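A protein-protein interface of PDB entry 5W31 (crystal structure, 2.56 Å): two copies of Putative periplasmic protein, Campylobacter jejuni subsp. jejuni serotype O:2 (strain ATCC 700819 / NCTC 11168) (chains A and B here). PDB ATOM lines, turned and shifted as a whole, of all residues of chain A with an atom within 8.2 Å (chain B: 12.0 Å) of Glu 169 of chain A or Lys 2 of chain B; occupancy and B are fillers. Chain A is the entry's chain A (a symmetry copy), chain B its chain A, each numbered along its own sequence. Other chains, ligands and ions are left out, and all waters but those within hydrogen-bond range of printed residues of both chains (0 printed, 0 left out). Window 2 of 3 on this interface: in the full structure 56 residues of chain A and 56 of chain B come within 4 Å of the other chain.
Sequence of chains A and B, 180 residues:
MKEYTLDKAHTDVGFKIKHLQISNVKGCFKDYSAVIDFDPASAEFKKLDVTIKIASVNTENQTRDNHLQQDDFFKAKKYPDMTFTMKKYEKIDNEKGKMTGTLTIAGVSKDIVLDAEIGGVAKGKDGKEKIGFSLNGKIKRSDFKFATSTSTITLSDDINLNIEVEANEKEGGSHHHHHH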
ATOM      1  N   VAL A  35      21.153 -24.868  10.488  1.00  0.00           N
ATOM      2  CA  VAL A  35      21.653 -23.509  10.300  1.00  0.00           C
ATOM      3  C   VAL A  35      20.435 -22.583  10.214  1.00  0.00           C
ATOM      4  O   VAL A  35      19.598 -22.714   9.321  1.00  0.00           O
ATOM      5  CB  VAL A  35      22.475 -23.422   8.985  1.00  0.00           C
ATOM      6  CG1 VAL A  35      22.888 -21.996   8.637  1.00  0.00           C
ATOM      7  CG2 VAL A  35      23.684 -24.347   9.046  1.00  0.00           C
ATOM      8  N   ILE A  36      20.351 -21.654  11.156  1.00  0.00           N
ATOM      9  CA  ILE A  36      19.257 -20.683  11.257  1.00  0.00           C
ATOM     10  C   ILE A  36      19.701 -19.187  11.149  1.00  0.00           C
ATOM     11  O   ILE A  36      20.355 -18.655  12.056  1.00  0.00           O
ATOM     12  CB  ILE A  36      18.502 -20.918  12.573  1.00  0.00           C
ATOM     13  CG1 ILE A  36      18.217 -22.409  12.764  1.00  0.00           C
ATOM     14  CG2 ILE A  36      17.231 -20.082  12.592  1.00  0.00           C
ATOM     15  CD1 ILE A  36      17.602 -22.771  14.109  1.00  0.00           C
ATOM     16  N   ASP A  37      19.348 -18.528  10.046  1.00  0.00           N
ATOM     17  CA  ASP A  37      19.533 -17.070   9.891  1.00  0.00           C
ATOM     18  C   ASP A  37      18.208 -16.323   9.918  1.00  0.00           C
ATOM     19  O   ASP A  37      17.358 -16.506   9.020  1.00  0.00           O
ATOM     20  CB  ASP A  37      20.221 -16.719   8.576  1.00  0.00           C
ATOM     21  CG  ASP A  37      21.686 -17.175   8.515  1.00  0.00           C
ATOM     22  OD1 ASP A  37      22.246 -17.696   9.534  1.00  0.00           O
ATOM     23  OD2 ASP A  37      22.268 -16.994   7.401  1.00  0.00           O
ATOM     24  N   PHE A  38      18.060 -15.452  10.914  1.00  0.00           N
ATOM     25  CA  PHE A  38      16.815 -14.727  11.149  1.00  0.00           C
ATOM     26  C   PHE A  38      17.047 -13.268  11.548  1.00  0.00           C
ATOM     27  O   PHE A  38      17.852 -12.994  12.427  1.00  0.00           O
ATOM     28  CB  PHE A  38      16.032 -15.458  12.248  1.00  0.00           C
ATOM     29  CG  PHE A  38      14.714 -14.841  12.579  1.00  0.00           C
ATOM     30  CD1 PHE A  38      13.616 -15.002  11.723  1.00  0.00           C
ATOM     31  CD2 PHE A  38      14.554 -14.105  13.767  1.00  0.00           C
ATOM     32  CE1 PHE A  38      12.386 -14.423  12.052  1.00  0.00           C
ATOM     33  CE2 PHE A  38      13.325 -13.525  14.096  1.00  0.00           C
ATOM     34  CZ  PHE A  38      12.242 -13.682  13.235  1.00  0.00           C
ATOM     35  N   ASP A  39      16.290 -12.358  10.938  1.00  0.00           N
ATOM     36  CA  ASP A  39      16.401 -10.900  11.160  1.00  0.00           C
ATOM     37  C   ASP A  39      15.293 -10.332  12.039  1.00  0.00           C
ATOM     38  O   ASP A  39      14.212  -9.977  11.515  1.00  0.00           O
ATOM     39  CB  ASP A  39      16.388 -10.146   9.816  1.00  0.00           C
ATOM     40  CG  ASP A  39      16.619  -8.658   9.968  1.00  0.00           C
ATOM     41  OD1 ASP A  39      17.215  -8.199  10.979  1.00  0.00           O
ATOM     42  OD2 ASP A  39      16.201  -7.938   9.048  1.00  0.00           O
ATOM     43  N   PRO A  40      15.569 -10.163  13.353  1.00  0.00           N
ATOM     44  CA  PRO A  40      14.537  -9.689  14.281  1.00  0.00           C
ATOM     45  C   PRO A  40      14.047  -8.276  13.992  1.00  0.00           C
ATOM     46  O   PRO A  40      12.963  -7.909  14.408  1.00  0.00           O
ATOM     47  CB  PRO A  40      15.223  -9.758  15.638  1.00  0.00           C
ATOM     48  CG  PRO A  40      16.455 -10.576  15.412  1.00  0.00           C
ATOM     49  CD  PRO A  40      16.867 -10.224  14.026  1.00  0.00           C
ATOM     50  N   ALA A  41      14.804  -7.494  13.241  1.00  0.00           N
ATOM     51  CA  ALA A  41      14.285  -6.196  12.796  1.00  0.00           C
ATOM     52  C   ALA A  41      13.026  -6.329  11.944  1.00  0.00           C
ATOM     53  O   ALA A  41      12.143  -5.480  12.001  1.00  0.00           O
ATOM     54  CB  ALA A  41      15.342  -5.395  12.040  1.00  0.00           C
ATOM     55  N   GLU A  44      11.905 -11.899   9.492  1.00  0.00           N
ATOM     56  CA  GLU A  44      12.119 -12.679   8.291  1.00  0.00           C
ATOM     57  C   GLU A  44      13.218 -13.703   8.485  1.00  0.00           C
ATOM     58  O   GLU A  44      14.249 -13.412   9.110  1.00  0.00           O
ATOM     59  CB  GLU A  44      12.479 -11.767   7.154  1.00  0.00           C
ATOM     60  CG  GLU A  44      11.295 -10.890   6.839  1.00  0.00           C
ATOM     61  CD  GLU A  44      11.498 -10.060   5.613  1.00  0.00           C
ATOM     62  OE1 GLU A  44      12.650  -9.655   5.353  1.00  0.00           O
ATOM     63  OE2 GLU A  44      10.499  -9.805   4.919  1.00  0.00           O
ATOM     64  N   PHE A  45      12.974 -14.918   7.985  1.00  0.00           N
ATOM     65  CA  PHE A  45      14.012 -15.931   7.933  1.00  0.00           C
ATOM     66  C   PHE A  45      14.808 -15.706   6.654  1.00  0.00           C
ATOM     67  O   PHE A  45      14.261 -15.242   5.612  1.00  0.00           O
ATOM     68  CB  PHE A  45      13.417 -17.302   7.984  1.00  0.00           C
ATOM     69  CG  PHE A  45      12.918 -17.714   9.353  1.00  0.00           C
ATOM     70  CD1 PHE A  45      11.610 -17.451   9.747  1.00  0.00           C
ATOM     71  CD2 PHE A  45      13.728 -18.436  10.221  1.00  0.00           C
ATOM     72  CE1 PHE A  45      11.129 -17.875  11.000  1.00  0.00           C
ATOM     73  CE2 PHE A  45      13.268 -18.868  11.477  1.00  0.00           C
ATOM     74  CZ  PHE A  45      11.959 -18.591  11.870  1.00  0.00           C
ATOM     75  N   LYS A  46      16.113 -15.967   6.748  1.00  0.00           N
ATOM     76  CA  LYS A  46      17.036 -15.697   5.612  1.00  0.00           C
ATOM     77  C   LYS A  46      17.597 -17.001   5.061  1.00  0.00           C
ATOM     78  O   LYS A  46      17.767 -17.153   3.845  1.00  0.00           O
ATOM     79  CB  LYS A  46      18.172 -14.725   6.009  1.00  0.00           C
ATOM     80  CG  LYS A  46      17.740 -13.322   6.476  1.00  0.00           C
ATOM     81  CD  LYS A  46      17.285 -12.459   5.301  1.00  0.00           C
ATOM     82  CE  LYS A  46      16.652 -11.162   5.765  1.00  0.00           C
ATOM     83  NZ  LYS A  46      16.304 -10.273   4.617  1.00  0.00           N
ATOM     84  N   LYS A  47      17.840 -17.942   5.974  1.00  0.00           N
ATOM     85  CA  LYS A  47      18.357 -19.243   5.652  1.00  0.00           C
ATOM     86  C   LYS A  47      17.871 -20.185   6.760  1.00  0.00           C
ATOM     87  O   LYS A  47      17.940 -19.865   7.958  1.00  0.00           O
ATOM     88  CB  LYS A  47      19.881 -19.147   5.637  1.00  0.00           C
ATOM     89  CG  LYS A  47      20.687 -20.265   5.005  1.00  0.00           C
ATOM     90  CD  LYS A  47      22.156 -20.104   5.406  1.00  0.00           C
ATOM     91  CE  LYS A  47      23.074 -21.169   4.818  1.00  0.00           C
ATOM     92  NZ  LYS A  47      23.290 -21.042   3.341  1.00  0.00           N
ATOM     93  N   ALA A 122      13.397 -12.232  21.608  1.00  0.00           N
ATOM     94  CA  ALA A 122      13.845 -11.680  22.889  1.00  0.00           C
ATOM     95  C   ALA A 122      15.359 -11.445  22.896  1.00  0.00           C
ATOM     96  O   ALA A 122      16.098 -12.021  22.069  1.00  0.00           O
ATOM     97  CB  ALA A 122      13.425 -12.617  24.039  1.00  0.00           C
ATOM     98  N   LYS A 123      15.806 -10.570  23.802  1.00  0.00           N
ATOM     99  CA  LYS A 123      17.197 -10.593  24.279  1.00  0.00           C
ATOM    100  C   LYS A 123      17.267 -11.401  25.581  1.00  0.00           C
ATOM    101  O   LYS A 123      16.515 -11.145  26.520  1.00  0.00           O
ATOM    102  CB  LYS A 123      17.754  -9.182  24.452  1.00  0.00           C
ATOM    103  CG  LYS A 123      18.590  -8.731  23.267  1.00  0.00           C
ATOM    104  CD  LYS A 123      18.410  -7.247  22.973  1.00  0.00           C
ATOM    105  CE  LYS A 123      19.183  -6.842  21.722  1.00  0.00           C
ATOM    106  NZ  LYS A 123      18.423  -5.832  20.920  1.00  0.00           N
ATOM    107  N   GLY A 124      18.153 -12.393  25.622  1.00  0.00           N
ATOM    108  CA  GLY A 124      18.215 -13.332  26.747  1.00  0.00           C
ATOM    109  C   GLY A 124      18.712 -12.722  28.049  1.00  0.00           C
ATOM    110  O   GLY A 124      19.022 -11.513  28.108  1.00  0.00           O
ATOM    111  N   ASP A 126      21.585 -12.890  29.437  1.00  0.00           N
ATOM    112  CA  ASP A 126      22.893 -12.288  29.158  1.00  0.00           C
ATOM    113  C   ASP A 126      22.940 -11.115  28.140  1.00  0.00           C
ATOM    114  O   ASP A 126      24.029 -10.661  27.794  1.00  0.00           O
ATOM    115  CB  ASP A 126      23.865 -13.406  28.717  1.00  0.00           C
ATOM    116  CG  ASP A 126      23.348 -14.212  27.504  1.00  0.00           C
ATOM    117  OD1 ASP A 126      22.234 -14.785  27.569  1.00  0.00           O
ATOM    118  OD2 ASP A 126      24.071 -14.287  26.487  1.00  0.00           O
ATOM    119  N   GLY A 127      21.791 -10.628  27.663  1.00  0.00           N
ATOM    120  CA  GLY A 127      21.774  -9.634  26.569  1.00  0.00           C
ATOM    121  C   GLY A 127      22.089 -10.119  25.137  1.00  0.00           C
ATOM    122  O   GLY A 127      22.196  -9.295  24.214  1.00  0.00           O
ATOM    123  N   LYS A 128      22.249 -11.438  24.947  1.00  0.00           N
ATOM    124  CA  LYS A 128      22.328 -12.070  23.609  1.00  0.00           C
ATOM    125  C   LYS A 128      20.973 -12.673  23.222  1.00  0.00           C
ATOM    126  O   LYS A 128      20.254 -13.217  24.083  1.00  0.00           O
ATOM    127  CB  LYS A 128      23.415 -13.150  23.560  1.00  0.00           C
ATOM    128  CG  LYS A 128      24.767 -12.667  23.045  1.00  0.00           C
ATOM    129  CD  LYS A 128      25.928 -13.229  23.867  1.00  0.00           C
ATOM    130  CE  LYS A 128      26.411 -14.599  23.403  1.00  0.00           C
ATOM    131  NZ  LYS A 128      27.340 -14.511  22.239  1.00  0.00           N
ATOM    132  N   GLU A 129      20.656 -12.588  21.927  1.00  0.00           N
ATOM    133  CA  GLU A 129      19.333 -12.942  21.359  1.00  0.00           C
ATOM    134  C   GLU A 129      18.838 -14.390  21.571  1.00  0.00           C
ATOM    135  O   GLU A 129      19.634 -15.355  21.620  1.00  0.00           O
ATOM    136  CB  GLU A 129      19.308 -12.654  19.843  1.00  0.00           C
ATOM    137  CG  GLU A 129      19.528 -11.206  19.405  1.00  0.00           C
ATOM    138  CD  GLU A 129      18.243 -10.422  19.204  1.00  0.00           C
ATOM    139  OE1 GLU A 129      18.361  -9.187  19.087  1.00  0.00           O
ATOM    140  OE2 GLU A 129      17.132 -11.020  19.141  1.00  0.00           O
ATOM    141  N   LYS A 130      17.517 -14.514  21.684  1.00  0.00           N
ATOM    142  CA  LYS A 130      16.829 -15.791  21.496  1.00  0.00           C
ATOM    143  C   LYS A 130      15.623 -15.649  20.552  1.00  0.00           C
ATOM    144  O   LYS A 130      15.265 -14.522  20.170  1.00  0.00           O
ATOM    145  CB  LYS A 130      16.477 -16.477  22.826  1.00  0.00           C
ATOM    146  CG  LYS A 130      15.880 -15.593  23.908  1.00  0.00           C
ATOM    147  CD  LYS A 130      15.914 -16.279  25.273  1.00  0.00           C
ATOM    148  CE  LYS A 130      15.043 -15.537  26.283  1.00  0.00           C
ATOM    149  NZ  LYS A 130      14.293 -16.477  27.173  1.00  0.00           N
ATOM    150  N   ILE A 131      15.090 -16.796  20.106  1.00  0.00           N
ATOM    151  CA  ILE A 131      13.840 -16.911  19.317  1.00  0.00           C
ATOM    152  C   ILE A 131      13.184 -18.221  19.640  1.00  0.00           C
ATOM    153  O   ILE A 131      13.866 -19.186  19.991  1.00  0.00           O
ATOM    154  CB  ILE A 131      13.992 -16.921  17.772  1.00  0.00           C
ATOM    155  CG1 ILE A 131      15.051 -17.924  17.323  1.00  0.00           C
ATOM    156  CG2 ILE A 131      14.240 -15.531  17.193  1.00  0.00           C
ATOM    157  CD1 ILE A 131      15.227 -17.920  15.823  1.00  0.00           C
ATOM    158  N   ALA A 167      15.959 -21.325  20.266  1.00  0.00           N
ATOM    159  CA  ALA A 167      17.279 -21.156  19.655  1.00  0.00           C
ATOM    160  C   ALA A 167      17.972 -19.839  20.062  1.00  0.00           C
ATOM    161  O   ALA A 167      17.341 -18.778  20.053  1.00  0.00           O
ATOM    162  CB  ALA A 167      17.179 -21.279  18.134  1.00  0.00           C
ATOM    163  N   ASN A 168      19.269 -19.923  20.392  1.00  0.00           N
ATOM    164  CA  ASN A 168      20.081 -18.792  20.887  1.00  0.00           C
ATOM    165  C   ASN A 168      21.087 -18.309  19.848  1.00  0.00           C
ATOM    166  O   ASN A 168      21.416 -19.040  18.909  1.00  0.00           O
ATOM    167  CB  ASN A 168      20.767 -19.186  22.183  1.00  0.00           C
ATOM    168  CG  ASN A 168      19.787 -19.735  23.209  1.00  0.00           C
ATOM    169  OD1 ASN A 168      19.088 -18.981  23.900  1.00  0.00           O
ATOM    170  ND2 ASN A 168      19.710 -21.061  23.300  1.00  0.00           N
ATOM    171  N   GLU A 169      21.549 -17.067  19.992  1.00  0.00           N
ATOM    172  CA  GLU A 169      22.478 -16.454  19.015  1.00  0.00           C
ATOM    173  C   GLU A 169      23.830 -17.207  18.959  1.00  0.00           C
ATOM    174  O   GLU A 169      24.108 -18.032  19.827  1.00  0.00           O
ATOM    175  CB  GLU A 169      22.679 -14.972  19.360  1.00  0.00           C
ATOM    176  CG  GLU A 169      22.987 -14.058  18.177  1.00  0.00           C
ATOM    177  CD  GLU A 169      23.240 -12.594  18.570  1.00  0.00           C
ATOM    178  OE1 GLU A 169      23.694 -11.819  17.685  1.00  0.00           O
ATOM    179  OE2 GLU A 169      22.986 -12.205  19.746  1.00  0.00           O
ATOM    180  N   LYS A 170      24.669 -16.917  17.961  1.00  0.00           N
ATOM    181  CA  LYS A 170      25.922 -17.663  17.743  1.00  0.00           C
ATOM    182  C   LYS A 170      27.208 -17.047  18.371  1.00  0.00           C
ATOM    183  O   LYS A 170      27.201 -15.873  18.773  1.00  0.00           O
ATOM    184  CB  LYS A 170      26.107 -17.946  16.241  1.00  0.00           C
ATOM    185  CG  LYS A 170      26.201 -19.435  15.942  1.00  0.00           C
ATOM    186  CD  LYS A 170      26.991 -19.749  14.687  1.00  0.00           C
ATOM    187  CE  LYS A 170      27.489 -21.190  14.815  1.00  0.00           C
ATOM    188  NZ  LYS A 170      28.362 -21.631  13.688  1.00  0.00           N
ATOM    189  N   GLU A 171      28.288 -17.856  18.434  1.00  0.00           N
ATOM    190  CA  GLU A 171      29.656 -17.498  18.933  1.00  0.00           C
ATOM    191  C   GLU A 171      29.656 -16.972  20.367  1.00  0.00           C
ATOM    192  O   GLU A 171      28.897 -17.457  21.209  1.00  0.00           O
ATOM    193  CB  GLU A 171      30.416 -16.537  17.983  1.00  0.00           C
ATOM    194  N   MET B   1      20.242  -9.235   9.901  1.00  0.00           N
ATOM    195  CA  MET B   1      20.353 -10.719   9.927  1.00  0.00           C
ATOM    196  C   MET B   1      21.174 -11.171  11.147  1.00  0.00           C
ATOM    197  O   MET B   1      22.007 -10.459  11.647  1.00  0.00           O
ATOM    198  CB  MET B   1      20.897 -11.222   8.579  1.00  0.00           C
ATOM    199  CG  MET B   1      20.911 -12.729   8.393  1.00  0.00           C
ATOM    200  SD  MET B   1      22.386 -13.492   9.124  1.00  0.00           S
ATOM    201  CE  MET B   1      23.629 -13.219   7.840  1.00  0.00           C
ATOM    202  N   LYS B   2      20.898 -12.360  11.639  1.00  0.00           N
ATOM    203  CA  LYS B   2      21.573 -12.884  12.810  1.00  0.00           C
ATOM    204  C   LYS B   2      21.557 -14.403  12.691  1.00  0.00           C
ATOM    205  O   LYS B   2      20.721 -14.970  11.984  1.00  0.00           O
ATOM    206  CB  LYS B   2      20.887 -12.407  14.099  1.00  0.00           C
ATOM    207  CG  LYS B   2      21.670 -11.355  14.832  1.00  0.00           C
ATOM    208  CD  LYS B   2      20.818 -10.152  15.210  1.00  0.00           C
ATOM    209  CE  LYS B   2      21.338  -9.441  16.468  1.00  0.00           C
ATOM    210  NZ  LYS B   2      22.759  -8.974  16.389  1.00  0.00           N
ATOM    211  N   GLU B   3      22.482 -15.056  13.377  1.00  0.00           N
ATOM    212  CA  GLU B   3      22.665 -16.484  13.238  1.00  0.00           C
ATOM    213  C   GLU B   3      22.347 -17.102  14.570  1.00  0.00           C
ATOM    214  O   GLU B   3      22.731 -16.567  15.616  1.00  0.00           O
ATOM    215  CB  GLU B   3      24.095 -16.819  12.822  1.00  0.00           C
ATOM    216  CG  GLU B   3      24.565 -16.111  11.554  1.00  0.00           C
ATOM    217  CD  GLU B   3      25.972 -16.514  11.126  1.00  0.00           C
ATOM    218  OE1 GLU B   3      26.634 -15.708  10.431  1.00  0.00           O
ATOM    219  OE2 GLU B   3      26.411 -17.638  11.472  1.00  0.00           O
ATOM    220  N   TYR B   4      21.620 -18.219  14.533  1.00  0.00           N
ATOM    221  CA  TYR B   4      21.191 -18.862  15.768  1.00  0.00           C
ATOM    222  C   TYR B   4      21.667 -20.304  15.807  1.00  0.00           C
ATOM    223  O   TYR B   4      22.112 -20.832  14.790  1.00  0.00           O
ATOM    224  CB  TYR B   4      19.672 -18.763  15.923  1.00  0.00           C
ATOM    225  CG  TYR B   4      19.131 -17.341  16.016  1.00  0.00           C
ATOM    226  CD1 TYR B   4      19.141 -16.457  14.884  1.00  0.00           C
ATOM    227  CD2 TYR B   4      18.563 -16.886  17.222  1.00  0.00           C
ATOM    228  CE1 TYR B   4      18.633 -15.161  14.973  1.00  0.00           C
ATOM    229  CE2 TYR B   4      18.042 -15.592  17.316  1.00  0.00           C
ATOM    230  CZ  TYR B   4      18.080 -14.734  16.204  1.00  0.00           C
ATOM    231  OH  TYR B   4      17.551 -13.467  16.358  1.00  0.00           O
ATOM    232  N   THR B   5      21.595 -20.914  16.983  1.00  0.00           N
ATOM    233  CA  THR B   5      22.013 -22.281  17.173  1.00  0.00           C
ATOM    234  C   THR B   5      20.871 -22.895  17.925  1.00  0.00           C
ATOM    235  O   THR B   5      20.485 -22.372  18.975  1.00  0.00           O
ATOM    236  CB  THR B   5      23.325 -22.379  18.026  1.00  0.00           C
ATOM    237  OG1 THR B   5      24.421 -21.815  17.296  1.00  0.00           O
ATOM    238  CG2 THR B   5      23.683 -23.852  18.409  1.00  0.00           C
ATOM    239  N   LEU B   6      20.343 -24.005  17.423  1.00  0.00           N
ATOM    240  CA  LEU B   6      19.265 -24.710  18.146  1.00  0.00           C
ATOM    241  C   LEU B   6      19.638 -24.980  19.589  1.00  0.00           C
ATOM    242  O   LEU B   6      20.814 -25.143  19.897  1.00  0.00           O
ATOM    243  CB  LEU B   6      18.925 -26.039  17.485  1.00  0.00           C
ATOM    244  CG  LEU B   6      18.279 -25.928  16.123  1.00  0.00           C
ATOM    245  CD1 LEU B   6      19.270 -26.384  15.068  1.00  0.00           C
ATOM    246  CD2 LEU B   6      17.072 -26.829  16.163  1.00  0.00           C
ATOM    247  N   ASP B   7      18.647 -24.988  20.468  1.00  0.00           N
ATOM    248  CA  ASP B   7      18.825 -25.520  21.805  1.00  0.00           C
ATOM    249  C   ASP B   7      18.062 -26.832  21.776  1.00  0.00           C
ATOM    250  O   ASP B   7      16.861 -26.882  22.063  1.00  0.00           O
ATOM    251  CB  ASP B   7      18.353 -24.526  22.897  1.00  0.00           C
ATOM    252  CG  ASP B   7      18.065 -25.197  24.274  1.00  0.00           C
ATOM    253  OD1 ASP B   7      18.568 -26.318  24.556  1.00  0.00           O
ATOM    254  OD2 ASP B   7      17.316 -24.587  25.086  1.00  0.00           O
ATOM    255  N   LYS B   8      18.782 -27.894  21.408  1.00  0.00           N
ATOM    256  CA  LYS B   8      18.222 -29.248  21.246  1.00  0.00           C
ATOM    257  C   LYS B   8      17.358 -29.701  22.438  1.00  0.00           C
ATOM    258  O   LYS B   8      16.444 -30.523  22.266  1.00  0.00           O
ATOM    259  CB  LYS B   8      19.322 -30.281  20.932  1.00  0.00           C
ATOM    260  CG  LYS B   8      20.182 -29.996  19.693  1.00  0.00           C
ATOM    261  CD  LYS B   8      20.142 -31.185  18.736  1.00  0.00           C
ATOM    262  CE  LYS B   8      21.503 -31.672  18.244  1.00  0.00           C
ATOM    263  NZ  LYS B   8      22.126 -30.734  17.275  1.00  0.00           N
ATOM    264  N   THR B  11      13.855 -28.066  21.880  1.00  0.00           N
ATOM    265  CA  THR B  11      13.458 -28.244  20.483  1.00  0.00           C
ATOM    266  C   THR B  11      12.914 -29.669  20.309  1.00  0.00           C
ATOM    267  O   THR B  11      13.403 -30.619  20.937  1.00  0.00           O
ATOM    268  CB  THR B  11      14.625 -27.924  19.519  1.00  0.00           C
ATOM    269  OG1 THR B  11      14.933 -26.527  19.599  1.00  0.00           O
ATOM    270  CG2 THR B  11      14.286 -28.239  18.073  1.00  0.00           C
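Asp 37 of chain A touches three residues of chain B.
Of the printed residues of chain B, Phe 38 of chain A touches Met 1, Lys 2 and Tyr 4.
Of chain B, only Met 1 (3.4 Å) comes within 4 Å of Asp 39 of chain A.
Printed residues of chain B within 4 Å of Pro 40 of chain A: Tyr 4 (3.2 Å).
Phe 45 of chain A touches none of the printed residues of chain B.
No residue of chain B comes within 4 Å of Lys 128 of chain A.
Glu 129 of chain A touches just these residues of chain B: Lys 2 and Tyr 4.
Asn 168 of chain A touches three residues of chain B.
Of chain B, only Lys 2 (3.3 Å) and Glu 3 (3.4 Å) come within 4 Å of Glu 169 of chain A.
No residue of chain B comes within 4 Å of Glu 171 of chain A.
Of chain A, only Ile 36, Asp 37, Phe 38, Glu 129 and Glu 169 come within 4 Å of Lys 2 of chain B.
The nearest printed residue of chain A that does not touch Thr 5 of chain B is Glu 169 of chain A (4.6 Å).
No position is printed for both chains.
O of Asp 7 of chain B is in hydrogen-bond range of OG1 of Thr 11 of chain B.
The backbone carbonyl oxygen (O) of Lys 47 of chain A sits at hydrogen-bond distance from the backbone NH (N) of Asp 37 of chain A, at 2.9 Å.
OD1 of Asp 39 of chain A lies close to N of Ala 41 of chain A.
N of Asp 39 of chain A lies within hydrogen-bond range of O of Glu 44 of chain A.
The backbone NH (N) of Glu 169 of chain A lies within hydrogen-bond range of the backbone carbonyl oxygen (O) of Glu 129 of chain A, 3.0 Å away.
O of Ala 167 of chain A lies within hydrogen-bond range of N of Ile 131 of chain A (3.0 Å).
Printed residues of chain B that touch a printed residue of chain A: Met 1, Lys 2, Glu 3, Tyr 4, Thr 5, Leu 6 and Asp 7.
Hydrophobic or aromatic side chains of chain B within 4 Å of the printed part of chain A: Met 1, Tyr 4 and Leu 6.
Along chain A the printed residues that touch a printed residue of chain B span positions 36 to 170.
Among the printed residues, 25 pairs touch across the chains.
Among the printed residues, Asp or Glu carboxylates within 4 Å of a Lys or Arg side-chain nitrogen of the other chain: Glu 169 of chain A with Lys 2 of chain B (3.3 Å).
The backbone NH (N) of Met 1 of chain B lies within hydrogen-bond range of the side-chain carboxylate (OD1) of Asp 39 of chain A.
O of Lys 2 of chain B is in hydrogen-bond range of N of Phe 38 of chain A (2.9 Å).
The side-chain carboxylate (OE1) of Glu 169 of chain A lies within salt-bridge range of the side-chain amino group (NZ) of Lys 2 of chain B (3.3 Å).
The backbone NH (N) of Lys 170 of chain A is in hydrogen-bond range of the backbone carbonyl oxygen (O) of Glu 3 of chain B (3.1 Å).
N of Tyr 4 of chain B lies within hydrogen-bond range of O of Ile 36 of chain A (2.8 Å).
N of Thr 5 of chain B is in hydrogen-bond range of O of Asn 168 of chain A (2.7 Å).
Among the printed residues, merely in contact across the chains: Asn 168 of chain A with Tyr 4 of chain B (3.2 Å), Asp 37 of chain A with Lys 2 of chain B (3.2 Å), Pro 40 of chain A with Tyr 4 of chain B (3.2 Å), Lys 170 of chain A with Thr 5 of chain B (3.3 Å), Ile 36 of chain A with Glu 3 of chain B (3.4 Å), Glu 169 of chain A with Glu 3 of chain B (3.4 Å), Phe 38 of chain A with Tyr 4 of chain B (3.4 Å), Asp 37 of chain A with Glu 3 of chain B (3.5 Å), Ala 167 of chain A with Thr 5 of chain B (3.5 Å), Ala 167 of chain A with Tyr 4 of chain B (3.6 Å), Ile 131 of chain A with Tyr 4 of chain B (3.7 Å), Ile 36 of chain A with Lys 2 of chain B (3.7 Å), Glu 129 of chain A with Tyr 4 of chain B (3.7 Å), Asn 168 of chain A with Asp 7 of chain B (3.7 Å), Lys 46 of chain A with Met 1 of chain B (3.8 Å), Asp 37 of chain A with Met 1 of chain B (3.8 Å), Ile 36 of chain A with Leu 6 of chain B (3.8 Å), Glu 129 of chain A with Lys 2 of chain B (3.9 Å) and Phe 38 of chain A with Met 1 of chain B (3.9997 Å).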
